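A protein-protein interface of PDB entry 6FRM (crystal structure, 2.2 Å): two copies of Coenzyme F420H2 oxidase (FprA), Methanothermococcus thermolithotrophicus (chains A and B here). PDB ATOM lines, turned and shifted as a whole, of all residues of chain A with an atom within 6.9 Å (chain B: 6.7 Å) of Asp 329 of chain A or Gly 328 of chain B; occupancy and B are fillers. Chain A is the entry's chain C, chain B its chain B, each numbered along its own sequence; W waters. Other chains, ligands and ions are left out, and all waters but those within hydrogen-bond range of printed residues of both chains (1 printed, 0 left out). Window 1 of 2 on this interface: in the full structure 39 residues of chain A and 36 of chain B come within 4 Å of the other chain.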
ATOM      1  N   LEU A 294      35.217 -29.867  16.256  1.00  0.00           N
ATOM      2  CA  LEU A 294      34.988 -29.332  17.607  1.00  0.00           C
ATOM      3  C   LEU A 294      36.244 -29.141  18.458  1.00  0.00           C
ATOM      4  O   LEU A 294      36.189 -28.401  19.441  1.00  0.00           O
ATOM      5  CB  LEU A 294      33.941 -30.138  18.383  1.00  0.00           C
ATOM      6  CG  LEU A 294      32.496 -29.944  17.948  1.00  0.00           C
ATOM      7  CD1 LEU A 294      31.603 -30.982  18.598  1.00  0.00           C
ATOM      8  CD2 LEU A 294      31.977 -28.526  18.261  1.00  0.00           C
ATOM      9  N   GLU A 298      34.088 -23.402  17.127  1.00  0.00           N
ATOM     10  CA  GLU A 298      33.152 -23.113  18.207  1.00  0.00           C
ATOM     11  C   GLU A 298      31.707 -22.926  17.732  1.00  0.00           C
ATOM     12  O   GLU A 298      31.438 -22.747  16.545  1.00  0.00           O
ATOM     13  CB  GLU A 298      33.660 -21.953  19.100  1.00  0.00           C
ATOM     14  CG  GLU A 298      34.063 -20.690  18.352  1.00  0.00           C
ATOM     15  CD  GLU A 298      32.842 -19.964  17.837  1.00  0.00           C
ATOM     16  OE1 GLU A 298      31.975 -19.590  18.666  1.00  0.00           O
ATOM     17  OE2 GLU A 298      32.678 -19.926  16.597  1.00  0.00           O
ATOM     18  N   ARG A 299      30.779 -23.007  18.693  1.00  0.00           N
ATOM     19  CA  ARG A 299      29.330 -22.966  18.519  1.00  0.00           C
ATOM     20  C   ARG A 299      28.724 -21.817  17.700  1.00  0.00           C
ATOM     21  O   ARG A 299      27.772 -22.093  16.973  1.00  0.00           O
ATOM     22  CB  ARG A 299      28.622 -23.035  19.876  1.00  0.00           C
ATOM     23  CG  ARG A 299      28.742 -21.778  20.727  1.00  0.00           C
ATOM     24  CD  ARG A 299      27.996 -21.948  22.025  1.00  0.00           C
ATOM     25  NE  ARG A 299      28.803 -22.560  23.082  1.00  0.00           N
ATOM     26  CZ  ARG A 299      29.680 -21.888  23.816  1.00  0.00           C
ATOM     27  NH1 ARG A 299      30.365 -22.499  24.772  1.00  0.00           N
ATOM     28  NH2 ARG A 299      29.904 -20.614  23.582  1.00  0.00           N
ATOM     29  N   PRO A 325      32.407 -35.641  24.948  1.00  0.00           N
ATOM     30  CA  PRO A 325      31.685 -34.554  25.637  1.00  0.00           C
ATOM     31  C   PRO A 325      31.523 -33.216  24.952  1.00  0.00           C
ATOM     32  O   PRO A 325      30.571 -32.520  25.295  1.00  0.00           O
ATOM     33  CB  PRO A 325      32.438 -34.399  26.953  1.00  0.00           C
ATOM     34  CG  PRO A 325      33.757 -35.072  26.739  1.00  0.00           C
ATOM     35  CD  PRO A 325      33.455 -36.207  25.831  1.00  0.00           C
ATOM     36  N   SER A 326      32.411 -32.840  24.014  1.00  0.00           N
ATOM     37  CA  SER A 326      32.342 -31.556  23.306  1.00  0.00           C
ATOM     38  C   SER A 326      30.990 -31.349  22.597  1.00  0.00           C
ATOM     39  O   SER A 326      30.566 -30.217  22.420  1.00  0.00           O
ATOM     40  CB  SER A 326      33.484 -31.449  22.299  1.00  0.00           C
ATOM     41  OG  SER A 326      33.388 -32.567  21.429  1.00  0.00           O
ATOM     42  N   VAL A 327      30.317 -32.443  22.196  1.00  0.00           N
ATOM     43  CA  VAL A 327      29.010 -32.354  21.528  1.00  0.00           C
ATOM     44  C   VAL A 327      27.938 -31.819  22.487  1.00  0.00           C
ATOM     45  O   VAL A 327      26.986 -31.198  22.032  1.00  0.00           O
ATOM     46  CB  VAL A 327      28.559 -33.665  20.816  1.00  0.00           C
ATOM     47  CG1 VAL A 327      29.610 -34.136  19.825  1.00  0.00           C
ATOM     48  CG2 VAL A 327      28.200 -34.769  21.824  1.00  0.00           C
ATOM     49  N   GLY A 328      28.116 -32.065  23.787  1.00  0.00           N
ATOM     50  CA  GLY A 328      27.214 -31.640  24.851  1.00  0.00           C
ATOM     51  C   GLY A 328      26.974 -30.152  24.851  1.00  0.00           C
ATOM     52  O   GLY A 328      25.846 -29.710  25.040  1.00  0.00           O
ATOM     53  N   ASP A 329      28.042 -29.366  24.618  1.00  0.00           N
ATOM     54  CA  ASP A 329      27.984 -27.926  24.559  1.00  0.00           C
ATOM     55  C   ASP A 329      27.127 -27.497  23.348  1.00  0.00           C
ATOM     56  O   ASP A 329      26.209 -26.695  23.508  1.00  0.00           O
ATOM     57  CB  ASP A 329      29.413 -27.340  24.476  1.00  0.00           C
ATOM     58  CG  ASP A 329      29.457 -25.832  24.367  1.00  0.00           C
ATOM     59  OD1 ASP A 329      28.826 -25.291  23.443  1.00  0.00           O
ATOM     60  OD2 ASP A 329      30.167 -25.199  25.175  1.00  0.00           O
ATOM     61  N   LEU A 330      27.423 -28.015  22.152  1.00  0.00           N
ATOM     62  CA  LEU A 330      26.658 -27.673  20.952  1.00  0.00           C
ATOM     63  C   LEU A 330      25.177 -28.086  21.078  1.00  0.00           C
ATOM     64  O   LEU A 330      24.303 -27.304  20.719  1.00  0.00           O
ATOM     65  CB  LEU A 330      27.308 -28.265  19.693  1.00  0.00           C
ATOM     66  CG  LEU A 330      26.614 -27.967  18.345  1.00  0.00           C
ATOM     67  CD1 LEU A 330      26.544 -26.481  18.049  1.00  0.00           C
ATOM     68  CD2 LEU A 330      27.289 -28.712  17.227  1.00  0.00           C
ATOM     69  N   ILE A 331      24.915 -29.277  21.619  1.00  0.00           N
ATOM     70  CA  ILE A 331      23.550 -29.803  21.822  1.00  0.00           C
ATOM     71  C   ILE A 331      22.764 -28.871  22.761  1.00  0.00           C
ATOM     72  O   ILE A 331      21.618 -28.530  22.461  1.00  0.00           O
ATOM     73  CB  ILE A 331      23.559 -31.303  22.270  1.00  0.00           C
ATOM     74  CG1 ILE A 331      23.984 -32.210  21.105  1.00  0.00           C
ATOM     75  CG2 ILE A 331      22.192 -31.726  22.842  1.00  0.00           C
ATOM     76  CD1 ILE A 331      24.422 -33.647  21.507  1.00  0.00           C
ATOM     77  N   TYR A 332      23.378 -28.449  23.874  1.00  0.00           N
ATOM     78  CA  TYR A 332      22.735 -27.537  24.839  1.00  0.00           C
ATOM     79  C   TYR A 332      22.396 -26.199  24.182  1.00  0.00           C
ATOM     80  O   TYR A 332      21.346 -25.621  24.475  1.00  0.00           O
ATOM     81  CB  TYR A 332      23.606 -27.344  26.101  1.00  0.00           C
ATOM     82  CG  TYR A 332      23.340 -28.372  27.186  1.00  0.00           C
ATOM     83  CD1 TYR A 332      23.276 -29.730  26.888  1.00  0.00           C
ATOM     84  CD2 TYR A 332      23.169 -27.987  28.514  1.00  0.00           C
ATOM     85  CE1 TYR A 332      23.014 -30.678  27.874  1.00  0.00           C
ATOM     86  CE2 TYR A 332      22.911 -28.931  29.511  1.00  0.00           C
ATOM     87  CZ  TYR A 332      22.847 -30.274  29.185  1.00  0.00           C
ATOM     88  OH  TYR A 332      22.620 -31.215  30.159  1.00  0.00           O
ATOM     89  N   TYR A 333      23.269 -25.730  23.283  1.00  0.00           N
ATOM     90  CA  TYR A 333      23.075 -24.472  22.551  1.00  0.00           C
ATOM     91  C   TYR A 333      21.892 -24.632  21.594  1.00  0.00           C
ATOM     92  O   TYR A 333      20.980 -23.805  21.609  1.00  0.00           O
ATOM     93  CB  TYR A 333      24.338 -24.113  21.779  1.00  0.00           C
ATOM     94  CG  TYR A 333      24.480 -22.657  21.412  1.00  0.00           C
ATOM     95  CD1 TYR A 333      24.193 -21.656  22.333  1.00  0.00           C
ATOM     96  CD2 TYR A 333      24.984 -22.281  20.174  1.00  0.00           C
ATOM     97  CE1 TYR A 333      24.365 -20.312  22.016  1.00  0.00           C
ATOM     98  CE2 TYR A 333      25.179 -20.942  19.850  1.00  0.00           C
ATOM     99  CZ  TYR A 333      24.860 -19.961  20.772  1.00  0.00           C
ATOM    100  OH  TYR A 333      25.035 -18.646  20.471  1.00  0.00           O
ATOM    101  N   LEU A 334      21.902 -25.712  20.789  1.00  0.00           N
ATOM    102  CA  LEU A 334      20.843 -26.046  19.816  1.00  0.00           C
ATOM    103  C   LEU A 334      19.482 -26.235  20.495  1.00  0.00           C
ATOM    104  O   LEU A 334      18.465 -25.907  19.910  1.00  0.00           O
ATOM    105  CB  LEU A 334      21.218 -27.292  18.993  1.00  0.00           C
ATOM    106  CG  LEU A 334      22.403 -27.126  18.026  1.00  0.00           C
ATOM    107  CD1 LEU A 334      22.852 -28.464  17.501  1.00  0.00           C
ATOM    108  CD2 LEU A 334      22.051 -26.201  16.865  1.00  0.00           C
ATOM    109  N   LEU B 294      34.200 -22.103  33.785  1.00  0.00           N
ATOM    110  CA  LEU B 294      34.118 -22.822  32.499  1.00  0.00           C
ATOM    111  C   LEU B 294      34.556 -22.022  31.277  1.00  0.00           C
ATOM    112  O   LEU B 294      34.856 -22.617  30.249  1.00  0.00           O
ATOM    113  CB  LEU B 294      32.736 -23.426  32.263  1.00  0.00           C
ATOM    114  CG  LEU B 294      32.391 -24.658  33.099  1.00  0.00           C
ATOM    115  CD1 LEU B 294      30.937 -24.986  32.974  1.00  0.00           C
ATOM    116  CD2 LEU B 294      33.208 -25.871  32.664  1.00  0.00           C
ATOM    117  N   PRO B 323      20.418 -23.746  30.601  1.00  0.00           N
ATOM    118  CA  PRO B 323      21.605 -23.234  31.275  1.00  0.00           C
ATOM    119  C   PRO B 323      22.670 -22.904  30.195  1.00  0.00           C
ATOM    120  O   PRO B 323      22.628 -23.522  29.105  1.00  0.00           O
ATOM    121  CB  PRO B 323      22.047 -24.401  32.170  1.00  0.00           C
ATOM    122  CG  PRO B 323      21.488 -25.608  31.544  1.00  0.00           C
ATOM    123  CD  PRO B 323      20.252 -25.203  30.812  1.00  0.00           C
ATOM    124  N   PHE B 324      23.622 -21.962  30.478  1.00  0.00           N
ATOM    125  CA  PHE B 324      24.693 -21.585  29.532  1.00  0.00           C
ATOM    126  C   PHE B 324      25.257 -22.873  28.923  1.00  0.00           C
ATOM    127  O   PHE B 324      25.484 -23.815  29.684  1.00  0.00           O
ATOM    128  CB  PHE B 324      25.762 -20.678  30.177  1.00  0.00           C
ATOM    129  CG  PHE B 324      26.619 -20.021  29.112  1.00  0.00           C
ATOM    130  CD1 PHE B 324      26.161 -18.914  28.415  1.00  0.00           C
ATOM    131  CD2 PHE B 324      27.862 -20.539  28.783  1.00  0.00           C
ATOM    132  CE1 PHE B 324      26.944 -18.326  27.416  1.00  0.00           C
ATOM    133  CE2 PHE B 324      28.638 -19.961  27.782  1.00  0.00           C
ATOM    134  CZ  PHE B 324      28.182 -18.852  27.111  1.00  0.00           C
ATOM    135  N   PRO B 325      25.415 -22.972  27.571  1.00  0.00           N
ATOM    136  CA  PRO B 325      25.786 -24.268  26.942  1.00  0.00           C
ATOM    137  C   PRO B 325      27.062 -24.987  27.393  1.00  0.00           C
ATOM    138  O   PRO B 325      27.149 -26.197  27.173  1.00  0.00           O
ATOM    139  CB  PRO B 325      25.850 -23.936  25.451  1.00  0.00           C
ATOM    140  CG  PRO B 325      26.036 -22.431  25.406  1.00  0.00           C
ATOM    141  CD  PRO B 325      25.156 -21.960  26.531  1.00  0.00           C
ATOM    142  N   SER B 326      28.018 -24.284  28.011  1.00  0.00           N
ATOM    143  CA  SER B 326      29.268 -24.899  28.463  1.00  0.00           C
ATOM    144  C   SER B 326      29.049 -26.020  29.493  1.00  0.00           C
ATOM    145  O   SER B 326      29.823 -26.977  29.520  1.00  0.00           O
ATOM    146  CB  SER B 326      30.238 -23.842  28.968  1.00  0.00           C
ATOM    147  OG  SER B 326      29.668 -23.145  30.062  1.00  0.00           O
ATOM    148  N   VAL B 327      27.972 -25.928  30.303  1.00  0.00           N
ATOM    149  CA  VAL B 327      27.628 -26.947  31.308  1.00  0.00           C
ATOM    150  C   VAL B 327      27.347 -28.276  30.637  1.00  0.00           C
ATOM    151  O   VAL B 327      27.545 -29.318  31.260  1.00  0.00           O
ATOM    152  CB  VAL B 327      26.481 -26.544  32.273  1.00  0.00           C
ATOM    153  CG1 VAL B 327      26.841 -25.307  33.090  1.00  0.00           C
ATOM    154  CG2 VAL B 327      25.171 -26.344  31.537  1.00  0.00           C
ATOM    155  N   GLY B 328      26.883 -28.226  29.378  1.00  0.00           N
ATOM    156  CA  GLY B 328      26.558 -29.402  28.577  1.00  0.00           C
ATOM    157  C   GLY B 328      27.731 -30.328  28.378  1.00  0.00           C
ATOM    158  O   GLY B 328      27.572 -31.532  28.487  1.00  0.00           O
ATOM    159  N   ASP B 329      28.918 -29.773  28.098  1.00  0.00           N
ATOM    160  CA  ASP B 329      30.150 -30.540  27.900  1.00  0.00           C
ATOM    161  C   ASP B 329      30.528 -31.287  29.222  1.00  0.00           C
ATOM    162  O   ASP B 329      30.811 -32.480  29.172  1.00  0.00           O
ATOM    163  CB  ASP B 329      31.297 -29.597  27.399  1.00  0.00           C
ATOM    164  CG  ASP B 329      32.670 -30.257  27.225  1.00  0.00           C
ATOM    165  OD1 ASP B 329      33.105 -30.981  28.140  1.00  0.00           O
ATOM    166  OD2 ASP B 329      33.279 -30.082  26.168  1.00  0.00           O
ATOM    167  N   LEU B 330      30.530 -30.588  30.390  1.00  0.00           N
ATOM    168  CA  LEU B 330      30.860 -31.193  31.674  1.00  0.00           C
ATOM    169  C   LEU B 330      29.807 -32.238  32.087  1.00  0.00           C
ATOM    170  O   LEU B 330      30.171 -33.300  32.579  1.00  0.00           O
ATOM    171  CB  LEU B 330      31.056 -30.130  32.753  1.00  0.00           C
ATOM    172  CG  LEU B 330      31.427 -30.627  34.173  1.00  0.00           C
ATOM    173  CD1 LEU B 330      32.758 -31.398  34.190  1.00  0.00           C
ATOM    174  CD2 LEU B 330      31.446 -29.476  35.147  1.00  0.00           C
ATOM    175  N   ILE B 331      28.518 -31.947  31.872  1.00  0.00           N
ATOM    176  CA  ILE B 331      27.418 -32.870  32.187  1.00  0.00           C
ATOM    177  C   ILE B 331      27.569 -34.183  31.373  1.00  0.00           C
ATOM    178  O   ILE B 331      27.444 -35.263  31.938  1.00  0.00           O
ATOM    179  CB  ILE B 331      26.020 -32.199  32.037  1.00  0.00           C
ATOM    180  CG1 ILE B 331      25.810 -31.146  33.172  1.00  0.00           C
ATOM    181  CG2 ILE B 331      24.888 -33.244  32.003  1.00  0.00           C
ATOM    182  CD1 ILE B 331      24.684 -30.121  32.952  1.00  0.00           C
ATOM    183  N   TYR B 332      27.882 -34.076  30.067  1.00  0.00           N
ATOM    184  CA  TYR B 332      28.082 -35.235  29.193  1.00  0.00           C
ATOM    185  C   TYR B 332      29.266 -36.059  29.684  1.00  0.00           C
ATOM    186  O   TYR B 332      29.202 -37.285  29.639  1.00  0.00           O
ATOM    187  CB  TYR B 332      28.262 -34.795  27.720  1.00  0.00           C
ATOM    188  CG  TYR B 332      26.961 -34.686  26.946  1.00  0.00           C
ATOM    189  CD1 TYR B 332      25.862 -34.020  27.478  1.00  0.00           C
ATOM    190  CD2 TYR B 332      26.834 -35.238  25.674  1.00  0.00           C
ATOM    191  CE1 TYR B 332      24.659 -33.929  26.779  1.00  0.00           C
ATOM    192  CE2 TYR B 332      25.642 -35.131  24.957  1.00  0.00           C
ATOM    193  CZ  TYR B 332      24.555 -34.481  25.518  1.00  0.00           C
ATOM    194  OH  TYR B 332      23.366 -34.381  24.836  1.00  0.00           O
ATOM    195  N   TYR B 333      30.331 -35.391  30.173  1.00  0.00           N
ATOM    196  CA  TYR B 333      31.522 -36.064  30.700  1.00  0.00           C
ATOM    197  C   TYR B 333      31.180 -36.804  31.988  1.00  0.00           C
ATOM    198  O   TYR B 333      31.495 -37.990  32.100  1.00  0.00           O
ATOM    199  CB  TYR B 333      32.630 -35.051  30.959  1.00  0.00           C
ATOM    200  CG  TYR B 333      34.037 -35.602  30.978  1.00  0.00           C
ATOM    201  CD1 TYR B 333      34.461 -36.523  30.023  1.00  0.00           C
ATOM    202  CD2 TYR B 333      34.972 -35.149  31.910  1.00  0.00           C
ATOM    203  CE1 TYR B 333      35.771 -36.992  30.002  1.00  0.00           C
ATOM    204  CE2 TYR B 333      36.287 -35.617  31.904  1.00  0.00           C
ATOM    205  CZ  TYR B 333      36.682 -36.539  30.947  1.00  0.00           C
ATOM    206  OH  TYR B 333      37.973 -37.010  30.923  1.00  0.00           O
HETATM  207  O   HOH W   1      22.245 -23.464  26.405  1.00  0.00           O
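The side-chain carboxylate of Asp 329 of chain A is in salt-bridge range of the guanidinium group of Arg 299 of chain A (2.7 Å).
Among the printed residues, merely in contact across the chains: Arg 299 of chain A with Pro 325 of chain B, Pro 325 of chain A with Asp 329 of chain B, Pro 325 of chain A with Tyr 333 of chain B, Ser 326 of chain A with Asp 329 of chain B, Gly 328 of chain A with Gly 328 of chain B, Gly 328 of chain A with Asp 329 of chain B, Gly 328 of chain A with Tyr 332 of chain B, Asp 329 of chain A with Pro 325 of chain B, Asp 329 of chain A with Ser 326 of chain B, Asp 329 of chain A with Gly 328 of chain B, Asp 329 of chain A with Asp 329 of chain B, Ile 331 of chain A with Tyr 332 of chain B, Tyr 332 of chain A with Pro 325 of chain B, Tyr 332 of chain A with Val 327 of chain B, Tyr 332 of chain A with Gly 328 of chain B, Tyr 332 of chain A with Ile 331 of chain B, Tyr 332 of chain A with Tyr 332 of chain B and Tyr 333 of chain A with Pro 325 of chain B.
Of chain B, only Pro 325, Ser 326, Gly 328 and Asp 329 come within 4 Å of Asp 329 of chain A. Of the printed residues of chain B, Ile 331 of chain A touches Tyr 332. Printed residues of chain B within 4 Å of Tyr 333 of chain A: Pro 325. Leu 294 of chain B touches none of the printed residues of chain A. Gly 328 of chain B touches just these residues of chain A: Gly 328, Asp 329 and Tyr 332. The nearest residue of chain B that does not touch Asp 329 of chain A is Val 327 of chain B (5.6 Å). The nearest printed residue of chain B that does not touch Tyr 332 of chain A is Pro 323 of chain B (4.1 Å).
Of the 13 printed residues of chain A, 8 touch a printed residue of chain B. Printed residues of chain B that touch a printed residue of chain A: Pro 325, Ser 326, Val 327, Gly 328, Asp 329, Ile 331, Tyr 332 and Tyr 333. Among the printed residues, 18 pairs touch across the chains.
Pro 325 of chain A touches Asp 329 of chain B, and with the chains exchanged Asp 329 of chain A touches Pro 325 of chain B. Gly 328 of chain A touches Asp 329 of chain B, and with the chains exchanged Asp 329 of chain A touches Gly 328 of chain B. Gly 328 of chain A touches Tyr 332 of chain B, and with the chains exchanged Tyr 332 of chain A touches Gly 328 of chain B. Tyr 332 of chain A touches Pro 325 of chain B, but with the chains exchanged Pro 325 of chain A does not touch Tyr 332 of chain B (4.01 Å). Positions printed for both chains: 294, 325, 326, 327, 328, 329, 330, 331, 332 and 333.
Water W1 bridges the backbone carbonyl oxygen of Pro 323 of chain B (2.7 Å) and the backbone carbonyl oxygen of Tyr 332 of chain A (3.0 Å).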
